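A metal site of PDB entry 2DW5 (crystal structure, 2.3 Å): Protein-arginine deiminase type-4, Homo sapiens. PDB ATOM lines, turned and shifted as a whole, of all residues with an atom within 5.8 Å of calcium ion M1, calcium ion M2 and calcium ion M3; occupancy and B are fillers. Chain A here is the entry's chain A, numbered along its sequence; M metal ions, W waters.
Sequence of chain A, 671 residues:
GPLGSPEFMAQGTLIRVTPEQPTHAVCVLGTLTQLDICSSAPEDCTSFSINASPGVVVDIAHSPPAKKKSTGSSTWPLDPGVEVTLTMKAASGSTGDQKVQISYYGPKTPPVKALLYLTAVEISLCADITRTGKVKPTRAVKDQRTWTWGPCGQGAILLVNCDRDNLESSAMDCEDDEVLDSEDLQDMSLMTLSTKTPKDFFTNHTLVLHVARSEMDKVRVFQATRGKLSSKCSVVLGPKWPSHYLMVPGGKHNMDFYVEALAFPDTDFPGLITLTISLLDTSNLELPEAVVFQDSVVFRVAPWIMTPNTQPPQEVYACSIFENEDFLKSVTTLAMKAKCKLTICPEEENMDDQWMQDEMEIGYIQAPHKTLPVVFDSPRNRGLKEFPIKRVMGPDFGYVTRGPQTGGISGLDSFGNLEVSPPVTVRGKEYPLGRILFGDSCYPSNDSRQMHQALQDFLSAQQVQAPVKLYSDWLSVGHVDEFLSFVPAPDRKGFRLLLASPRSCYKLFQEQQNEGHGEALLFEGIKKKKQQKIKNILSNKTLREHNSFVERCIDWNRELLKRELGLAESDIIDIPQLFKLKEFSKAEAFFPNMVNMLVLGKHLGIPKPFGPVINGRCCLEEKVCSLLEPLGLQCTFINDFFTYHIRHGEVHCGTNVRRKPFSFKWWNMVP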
ATOM      1  N   ASN A 161      21.285   5.877   4.009  1.00  0.00           N
ATOM      2  CA  ASN A 161      21.900   4.593   4.347  1.00  0.00           C
ATOM      3  C   ASN A 161      22.709   4.647   5.648  1.00  0.00           C
ATOM      4  O   ASN A 161      23.890   4.328   5.718  1.00  0.00           O
ATOM      5  CB  ASN A 161      22.668   4.020   3.153  1.00  0.00           C
ATOM      6  CG  ASN A 161      22.998   2.511   3.291  1.00  0.00           C
ATOM      7  OD1 ASN A 161      22.618   1.851   4.275  1.00  0.00           O
ATOM      8  ND2 ASN A 161      23.724   1.988   2.317  1.00  0.00           N
ATOM      9  N   CYS A 162      21.986   4.950   6.719  1.00  0.00           N
ATOM     10  CA  CYS A 162      22.548   5.384   7.981  1.00  0.00           C
ATOM     11  C   CYS A 162      22.553   4.293   9.027  1.00  0.00           C
ATOM     12  O   CYS A 162      22.698   4.590  10.215  1.00  0.00           O
ATOM     13  CB  CYS A 162      21.710   6.545   8.513  1.00  0.00           C
ATOM     14  SG  CYS A 162      20.016   6.077   8.862  1.00  0.00           S
ATOM     15  N   ASP A 163      22.352   3.046   8.587  1.00  0.00           N
ATOM     16  CA  ASP A 163      22.520   1.880   9.441  1.00  0.00           C
ATOM     17  C   ASP A 163      23.904   1.251   9.200  1.00  0.00           C
ATOM     18  O   ASP A 163      24.722   1.786   8.439  1.00  0.00           O
ATOM     19  CB  ASP A 163      21.363   0.882   9.252  1.00  0.00           C
ATOM     20  CG  ASP A 163      21.475   0.048   7.981  1.00  0.00           C
ATOM     21  OD1 ASP A 163      22.074   0.506   6.963  1.00  0.00           O
ATOM     22  OD2 ASP A 163      20.949  -1.102   8.023  1.00  0.00           O
ATOM     23  N   ARG A 164      24.159   0.136   9.887  1.00  0.00           N
ATOM     24  CA  ARG A 164      25.492  -0.503   9.879  1.00  0.00           C
ATOM     25  C   ARG A 164      25.364  -2.019   9.745  1.00  0.00           C
ATOM     26  O   ARG A 164      25.367  -2.750  10.733  1.00  0.00           O
ATOM     27  CB  ARG A 164      26.277  -0.154  11.146  1.00  0.00           C
ATOM     28  CG  ARG A 164      27.737  -0.553  11.121  1.00  0.00           C
ATOM     29  CD  ARG A 164      28.516   0.020  12.299  1.00  0.00           C
ATOM     30  NE  ARG A 164      28.465  -0.892  13.437  1.00  0.00           N
ATOM     31  CZ  ARG A 164      27.972  -0.610  14.650  1.00  0.00           C
ATOM     32  NH1 ARG A 164      27.485   0.588  14.967  1.00  0.00           N
ATOM     33  NH2 ARG A 164      27.982  -1.561  15.571  1.00  0.00           N
ATOM     34  N   ASP A 165      25.229  -2.478   8.496  1.00  0.00           N
ATOM     35  CA  ASP A 165      25.224  -3.903   8.167  1.00  0.00           C
ATOM     36  C   ASP A 165      26.631  -4.519   8.215  1.00  0.00           C
ATOM     37  O   ASP A 165      26.766  -5.732   8.376  1.00  0.00           O
ATOM     38  CB  ASP A 165      24.604  -4.146   6.764  1.00  0.00           C
ATOM     39  CG  ASP A 165      23.159  -3.657   6.655  1.00  0.00           C
ATOM     40  OD1 ASP A 165      22.302  -4.060   7.479  1.00  0.00           O
ATOM     41  OD2 ASP A 165      22.898  -2.858   5.739  1.00  0.00           O
ATOM     42  N   ASP A 173      26.973   2.673   6.965  1.00  0.00           N
ATOM     43  CA  ASP A 173      27.392   2.102   5.671  1.00  0.00           C
ATOM     44  C   ASP A 173      27.633   3.160   4.579  1.00  0.00           C
ATOM     45  O   ASP A 173      28.448   2.932   3.700  1.00  0.00           O
ATOM     46  CB  ASP A 173      26.379   1.084   5.148  1.00  0.00           C
ATOM     47  CG  ASP A 173      26.079  -0.053   6.135  1.00  0.00           C
ATOM     48  OD1 ASP A 173      27.009  -0.612   6.776  1.00  0.00           O
ATOM     49  OD2 ASP A 173      24.900  -0.395   6.259  1.00  0.00           O
ATOM     50  N   CYS A 174      26.909   4.297   4.623  1.00  0.00           N
ATOM     51  CA  CYS A 174      27.030   5.326   3.577  1.00  0.00           C
ATOM     52  C   CYS A 174      28.182   6.328   3.750  1.00  0.00           C
ATOM     53  O   CYS A 174      28.282   7.315   3.013  1.00  0.00           O
ATOM     54  CB  CYS A 174      25.727   6.108   3.421  1.00  0.00           C
ATOM     55  SG  CYS A 174      25.330   7.150   4.850  1.00  0.00           S
ATOM     56  N   GLU A 175      29.079   6.072   4.705  1.00  0.00           N
ATOM     57  CA  GLU A 175      30.209   6.977   4.881  1.00  0.00           C
ATOM     58  C   GLU A 175      31.399   6.650   3.946  1.00  0.00           C
ATOM     59  O   GLU A 175      32.263   7.512   3.746  1.00  0.00           O
ATOM     60  CB  GLU A 175      30.600   7.052   6.353  1.00  0.00           C
ATOM     61  CG  GLU A 175      29.559   7.833   7.163  1.00  0.00           C
ATOM     62  CD  GLU A 175      29.825   7.876   8.670  1.00  0.00           C
ATOM     63  OE1 GLU A 175      30.513   6.948   9.186  1.00  0.00           O
ATOM     64  OE2 GLU A 175      29.340   8.828   9.333  1.00  0.00           O
ATOM     65  N   ASP A 176      31.425   5.448   3.366  1.00  0.00           N
ATOM     66  CA  ASP A 176      32.449   5.079   2.371  1.00  0.00           C
ATOM     67  C   ASP A 176      31.793   5.021   1.006  1.00  0.00           C
ATOM     68  O   ASP A 176      30.555   5.243   0.888  1.00  0.00           O
ATOM     69  CB  ASP A 176      33.100   3.732   2.720  1.00  0.00           C
ATOM     70  CG  ASP A 176      32.138   2.546   2.621  1.00  0.00           C
ATOM     71  OD1 ASP A 176      32.417   1.487   3.219  1.00  0.00           O
ATOM     72  OD2 ASP A 176      31.086   2.640   1.942  1.00  0.00           O
ATOM     73  N   ASP A 177      32.585   4.704  -0.017  1.00  0.00           N
ATOM     74  CA  ASP A 177      32.069   4.618  -1.406  1.00  0.00           C
ATOM     75  C   ASP A 177      32.107   3.192  -1.943  1.00  0.00           C
ATOM     76  O   ASP A 177      32.582   2.936  -3.057  1.00  0.00           O
ATOM     77  CB  ASP A 177      32.779   5.602  -2.349  1.00  0.00           C
ATOM     78  CG  ASP A 177      34.181   5.947  -1.904  1.00  0.00           C
ATOM     79  OD1 ASP A 177      35.149   5.190  -2.222  1.00  0.00           O
ATOM     80  OD2 ASP A 177      34.325   7.003  -1.241  1.00  0.00           O
ATOM     81  N   GLU A 178      31.564   2.259  -1.156  1.00  0.00           N
ATOM     82  CA  GLU A 178      31.569   0.835  -1.482  1.00  0.00           C
ATOM     83  C   GLU A 178      30.364   0.095  -0.914  1.00  0.00           C
ATOM     84  O   GLU A 178      29.948   0.345   0.216  1.00  0.00           O
ATOM     85  CB  GLU A 178      32.810   0.209  -0.881  1.00  0.00           C
ATOM     86  CG  GLU A 178      34.085   0.692  -1.497  1.00  0.00           C
ATOM     87  CD  GLU A 178      35.251  -0.150  -1.059  1.00  0.00           C
ATOM     88  OE1 GLU A 178      35.203  -1.387  -1.273  1.00  0.00           O
ATOM     89  OE2 GLU A 178      36.212   0.429  -0.509  1.00  0.00           O
ATOM     90  N   VAL A 179      29.838  -0.860  -1.680  1.00  0.00           N
ATOM     91  CA  VAL A 179      28.841  -1.782  -1.150  1.00  0.00           C
ATOM     92  C   VAL A 179      29.630  -2.945  -0.536  1.00  0.00           C
ATOM     93  O   VAL A 179      30.141  -3.791  -1.276  1.00  0.00           O
ATOM     94  CB  VAL A 179      27.847  -2.277  -2.230  1.00  0.00           C
ATOM     95  CG1 VAL A 179      26.722  -3.088  -1.593  1.00  0.00           C
ATOM     96  CG2 VAL A 179      27.245  -1.119  -2.977  1.00  0.00           C
ATOM     97  N   LEU A 180      29.746  -2.971   0.787  1.00  0.00           N
ATOM     98  CA  LEU A 180      30.637  -3.950   1.472  1.00  0.00           C
ATOM     99  C   LEU A 180      29.969  -5.279   1.733  1.00  0.00           C
ATOM    100  O   LEU A 180      30.630  -6.306   1.823  1.00  0.00           O
ATOM    101  CB  LEU A 180      31.172  -3.406   2.800  1.00  0.00           C
ATOM    102  CG  LEU A 180      32.328  -2.414   2.695  1.00  0.00           C
ATOM    103  CD1 LEU A 180      32.773  -2.021   4.118  1.00  0.00           C
ATOM    104  CD2 LEU A 180      33.498  -2.950   1.830  1.00  0.00           C
ATOM    105  N   GLU A 183      23.763  -7.611   1.701  1.00  0.00           N
ATOM    106  CA  GLU A 183      22.597  -7.156   2.464  1.00  0.00           C
ATOM    107  C   GLU A 183      22.392  -5.640   2.424  1.00  0.00           C
ATOM    108  O   GLU A 183      21.272  -5.168   2.519  1.00  0.00           O
ATOM    109  CB  GLU A 183      22.703  -7.561   3.944  1.00  0.00           C
ATOM    110  CG  GLU A 183      22.612  -9.049   4.204  1.00  0.00           C
ATOM    111  CD  GLU A 183      23.950  -9.751   4.086  1.00  0.00           C
ATOM    112  OE1 GLU A 183      23.998 -10.942   4.450  1.00  0.00           O
ATOM    113  OE2 GLU A 183      24.937  -9.127   3.625  1.00  0.00           O
ATOM    114  N   ASP A 184      23.496  -4.902   2.313  1.00  0.00           N
ATOM    115  CA  ASP A 184      23.488  -3.448   2.254  1.00  0.00           C
ATOM    116  C   ASP A 184      22.626  -2.949   1.089  1.00  0.00           C
ATOM    117  O   ASP A 184      21.956  -1.895   1.221  1.00  0.00           O
ATOM    118  CB  ASP A 184      24.915  -2.881   2.138  1.00  0.00           C
ATOM    119  CG  ASP A 184      24.970  -1.334   2.167  1.00  0.00           C
ATOM    120  OD1 ASP A 184      25.733  -0.729   1.384  1.00  0.00           O
ATOM    121  OD2 ASP A 184      24.258  -0.710   2.979  1.00  0.00           O
ATOM    122  N   GLN A 186      19.875  -4.006   0.056  1.00  0.00           N
ATOM    123  CA  GLN A 186      18.472  -4.005   0.417  1.00  0.00           C
ATOM    124  C   GLN A 186      18.029  -2.647   0.913  1.00  0.00           C
ATOM    125  O   GLN A 186      16.848  -2.301   0.806  1.00  0.00           O
ATOM    126  CB  GLN A 186      18.200  -5.084   1.484  1.00  0.00           C
ATOM    127  CG  GLN A 186      18.453  -6.515   1.004  1.00  0.00           C
ATOM    128  CD  GLN A 186      18.447  -7.547   2.148  1.00  0.00           C
ATOM    129  OE1 GLN A 186      18.999  -8.656   2.006  1.00  0.00           O
ATOM    130  NE2 GLN A 186      17.833  -7.186   3.284  1.00  0.00           N
ATOM    131  N   ASP A 187      18.944  -1.866   1.463  1.00  0.00           N
ATOM    132  CA  ASP A 187      18.590  -0.511   1.890  1.00  0.00           C
ATOM    133  C   ASP A 187      18.552   0.444   0.718  1.00  0.00           C
ATOM    134  O   ASP A 187      17.962   1.508   0.831  1.00  0.00           O
ATOM    135  CB  ASP A 187      19.546   0.038   2.940  1.00  0.00           C
ATOM    136  CG  ASP A 187      19.612  -0.842   4.159  1.00  0.00           C
ATOM    137  OD1 ASP A 187      18.595  -1.452   4.576  1.00  0.00           O
ATOM    138  OD2 ASP A 187      20.718  -0.953   4.690  1.00  0.00           O
ATOM    139  N   MET A 188      19.146   0.044  -0.407  1.00  0.00           N
ATOM    140  CA  MET A 188      19.301   0.933  -1.561  1.00  0.00           C
ATOM    141  C   MET A 188      18.161   0.830  -2.549  1.00  0.00           C
ATOM    142  O   MET A 188      17.455  -0.144  -2.573  1.00  0.00           O
ATOM    143  CB  MET A 188      20.625   0.637  -2.252  1.00  0.00           C
ATOM    144  CG  MET A 188      21.772   0.786  -1.330  1.00  0.00           C
ATOM    145  SD  MET A 188      23.322   0.855  -2.211  1.00  0.00           S
ATOM    146  CE  MET A 188      24.411   0.529  -0.845  1.00  0.00           C
ATOM    147  N   ARG A 220      24.686   8.650  -3.445  1.00  0.00           N
ATOM    148  CA  ARG A 220      25.734   7.821  -4.050  1.00  0.00           C
ATOM    149  C   ARG A 220      25.071   6.763  -4.907  1.00  0.00           C
ATOM    150  O   ARG A 220      23.991   6.267  -4.560  1.00  0.00           O
ATOM    151  CB  ARG A 220      26.628   7.213  -2.997  1.00  0.00           C
ATOM    152  CG  ARG A 220      27.803   6.458  -3.622  1.00  0.00           C
ATOM    153  CD  ARG A 220      28.723   5.939  -2.612  1.00  0.00           C
ATOM    154  NE  ARG A 220      29.448   7.016  -1.965  1.00  0.00           N
ATOM    155  CZ  ARG A 220      29.261   7.440  -0.728  1.00  0.00           C
ATOM    156  NH1 ARG A 220      28.348   6.871   0.070  1.00  0.00           N
ATOM    157  NH2 ARG A 220      30.016   8.435  -0.254  1.00  0.00           N
ATOM    158  N   PHE A 222      25.737   3.254  -7.304  1.00  0.00           N
ATOM    159  CA  PHE A 222      26.609   2.143  -7.680  1.00  0.00           C
ATOM    160  C   PHE A 222      26.066   1.437  -8.931  1.00  0.00           C
ATOM    161  O   PHE A 222      24.865   1.343  -9.129  1.00  0.00           O
ATOM    162  CB  PHE A 222      26.692   1.112  -6.547  1.00  0.00           C
ATOM    163  CG  PHE A 222      27.270   1.651  -5.247  1.00  0.00           C
ATOM    164  CD1 PHE A 222      26.441   2.225  -4.269  1.00  0.00           C
ATOM    165  CD2 PHE A 222      28.636   1.563  -4.998  1.00  0.00           C
ATOM    166  CE1 PHE A 222      26.981   2.714  -3.056  1.00  0.00           C
ATOM    167  CE2 PHE A 222      29.167   2.060  -3.792  1.00  0.00           C
ATOM    168  CZ  PHE A 222      28.345   2.625  -2.831  1.00  0.00           C
ATOM    169  N   GLU A 260      21.723   5.212  -2.834  1.00  0.00           N
ATOM    170  CA  GLU A 260      21.562   5.423  -1.387  1.00  0.00           C
ATOM    171  C   GLU A 260      21.621   6.895  -1.165  1.00  0.00           C
ATOM    172  O   GLU A 260      22.365   7.574  -1.861  1.00  0.00           O
ATOM    173  CB  GLU A 260      22.704   4.750  -0.614  1.00  0.00           C
ATOM    174  CG  GLU A 260      24.145   5.136  -1.065  1.00  0.00           C
ATOM    175  CD  GLU A 260      25.209   4.540  -0.160  1.00  0.00           C
ATOM    176  OE1 GLU A 260      24.887   3.611   0.610  1.00  0.00           O
ATOM    177  OE2 GLU A 260      26.376   4.971  -0.189  1.00  0.00           O
ATOM    178  N   LYS A 370      11.779  -1.255   1.864  1.00  0.00           N
ATOM    179  CA  LYS A 370      12.562  -1.375   3.120  1.00  0.00           C
ATOM    180  C   LYS A 370      12.117  -0.340   4.176  1.00  0.00           C
ATOM    181  O   LYS A 370      12.023   0.855   3.910  1.00  0.00           O
ATOM    182  CB  LYS A 370      14.078  -1.213   2.834  1.00  0.00           C
ATOM    183  CG  LYS A 370      15.022  -1.643   3.988  1.00  0.00           C
ATOM    184  CD  LYS A 370      14.936  -3.167   4.243  1.00  0.00           C
ATOM    185  CE  LYS A 370      16.212  -3.774   4.862  1.00  0.00           C
ATOM    186  NZ  LYS A 370      16.488  -5.188   4.372  1.00  0.00           N
ATOM    187  N   LEU A 372      13.219   0.612   8.220  1.00  0.00           N
ATOM    188  CA  LEU A 372      14.073   0.256   9.359  1.00  0.00           C
ATOM    189  C   LEU A 372      14.012   1.226  10.501  1.00  0.00           C
ATOM    190  O   LEU A 372      13.730   2.389  10.291  1.00  0.00           O
ATOM    191  CB  LEU A 372      15.516   0.066   8.952  1.00  0.00           C
ATOM    192  CG  LEU A 372      16.287   1.127   8.200  1.00  0.00           C
ATOM    193  CD1 LEU A 372      17.692   1.296   8.815  1.00  0.00           C
ATOM    194  CD2 LEU A 372      16.404   0.667   6.784  1.00  0.00           C
ATOM    195  N   PRO A 395      22.991  -3.557  12.436  1.00  0.00           N
ATOM    196  CA  PRO A 395      22.273  -4.208  11.357  1.00  0.00           C
ATOM    197  C   PRO A 395      20.786  -3.912  11.373  1.00  0.00           C
ATOM    198  O   PRO A 395      20.076  -4.351  12.276  1.00  0.00           O
ATOM    199  CB  PRO A 395      22.539  -5.715  11.610  1.00  0.00           C
ATOM    200  CG  PRO A 395      23.864  -5.726  12.303  1.00  0.00           C
ATOM    201  CD  PRO A 395      23.756  -4.533  13.234  1.00  0.00           C
ATOM    202  N   ASP A 396      20.361  -3.161  10.364  1.00  0.00           N
ATOM    203  CA  ASP A 396      18.962  -2.738  10.211  1.00  0.00           C
ATOM    204  C   ASP A 396      18.494  -1.859  11.358  1.00  0.00           C
ATOM    205  O   ASP A 396      17.326  -1.856  11.746  1.00  0.00           O
ATOM    206  CB  ASP A 396      18.029  -3.921   9.909  1.00  0.00           C
ATOM    207  CG  ASP A 396      18.194  -4.429   8.466  1.00  0.00           C
ATOM    208  OD1 ASP A 396      18.474  -3.596   7.582  1.00  0.00           O
ATOM    209  OD2 ASP A 396      18.067  -5.644   8.196  1.00  0.00           O
HETATM  210 CA    CA M   1      20.178  -2.874   6.197  1.00  0.00          CA
HETATM  211 CA    CA M   2      22.934  -0.455   5.022  1.00  0.00          CA
HETATM  212 CA    CA M   3      28.972   1.709   1.805  1.00  0.00          CA
HETATM  213  O   HOH W   1      28.584   3.577   0.516  1.00  0.00           O
HETATM  214  O   HOH W   2      26.292   1.800   1.550  1.00  0.00           O
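Calcium ion M2 is bound by OD2 of Asp 187 (2.3 Å), OD2 of Asp 173 (2.3 Å), OD1 of Asp 163 (2.3 Å), OD1 of Asn 161 (2.4 Å), OD2 of Asp 184 (2.4 Å) and OD2 of Asp 165 (2.5 Å).
Three residues have an atom within 4 Å of calcium ion M3: Asp 173, Asp 176 and Glu 178.
The nearest printed residue that does not touch calcium ion M3 is Asp 184 (4.1 Å).
Of the 25 residues printed, 4 come within 4 Å of calcium ion M1.
The nearest printed residue that does not touch calcium ion M1 is Lys 370 (4.3 Å).
The nearest printed residue that does not touch calcium ion M2 is Arg 164 (5.1 Å).
Calcium ion M1 is bound by the side-chain carboxylate (OD1) of Asp 396 (2.3 Å), the side-chain carboxylate (OD2) of Asp 187 (2.5 Å), the side-chain carboxylate (OD2) of Asp 163 (2.7 Å), the side-chain carboxylate (OD1) of Asp 187 (2.7 Å), the side-chain carboxylate (OD1) of Asp 165 (2.7 Å) and the side-chain carboxylate (OD2) of Asp 165 (2.8 Å).
Water W1 binds calcium ion M3, 2.3 Å away.
O of Glu 178 binds calcium ion M3.
OD2 of Asp 176 is bound to calcium ion M3 (2.3 Å).
Calcium ion M3 is bound by O of Asp 173 (2.3 Å).
Calcium ion M3 is bound by water W2 (2.7 Å).
Calcium ion M3 has five donor atoms within binding distance.
The backbone carbonyl oxygen (O) of Asp 176 is in hydrogen-bond range of the guanidinium group (NH1) of Arg 220 (2.9 Å).
The backbone NH (N) of Cys 174 sits at hydrogen-bond distance from the backbone carbonyl oxygen (O) of Asn 161 (3.2 Å).
The side-chain carboxylate (OE1) of Glu 260 sits at hydrogen-bond distance from the side-chain amide nitrogen (ND2) of Asn 161 (2.6 Å).
Water W1 lies within hydrogen-bond range of the backbone carbonyl oxygen (O) of Asp 176, the side-chain carboxylate (OE2) of Glu 260 and the guanidinium group (NH1) of Arg 220.
Water W2 lies within hydrogen-bond range of the side-chain carboxylate (OE1) of Glu 260, the side-chain carboxylate (OD1) of Asp 184 and the side-chain amide nitrogen (ND2) of Asn 161.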
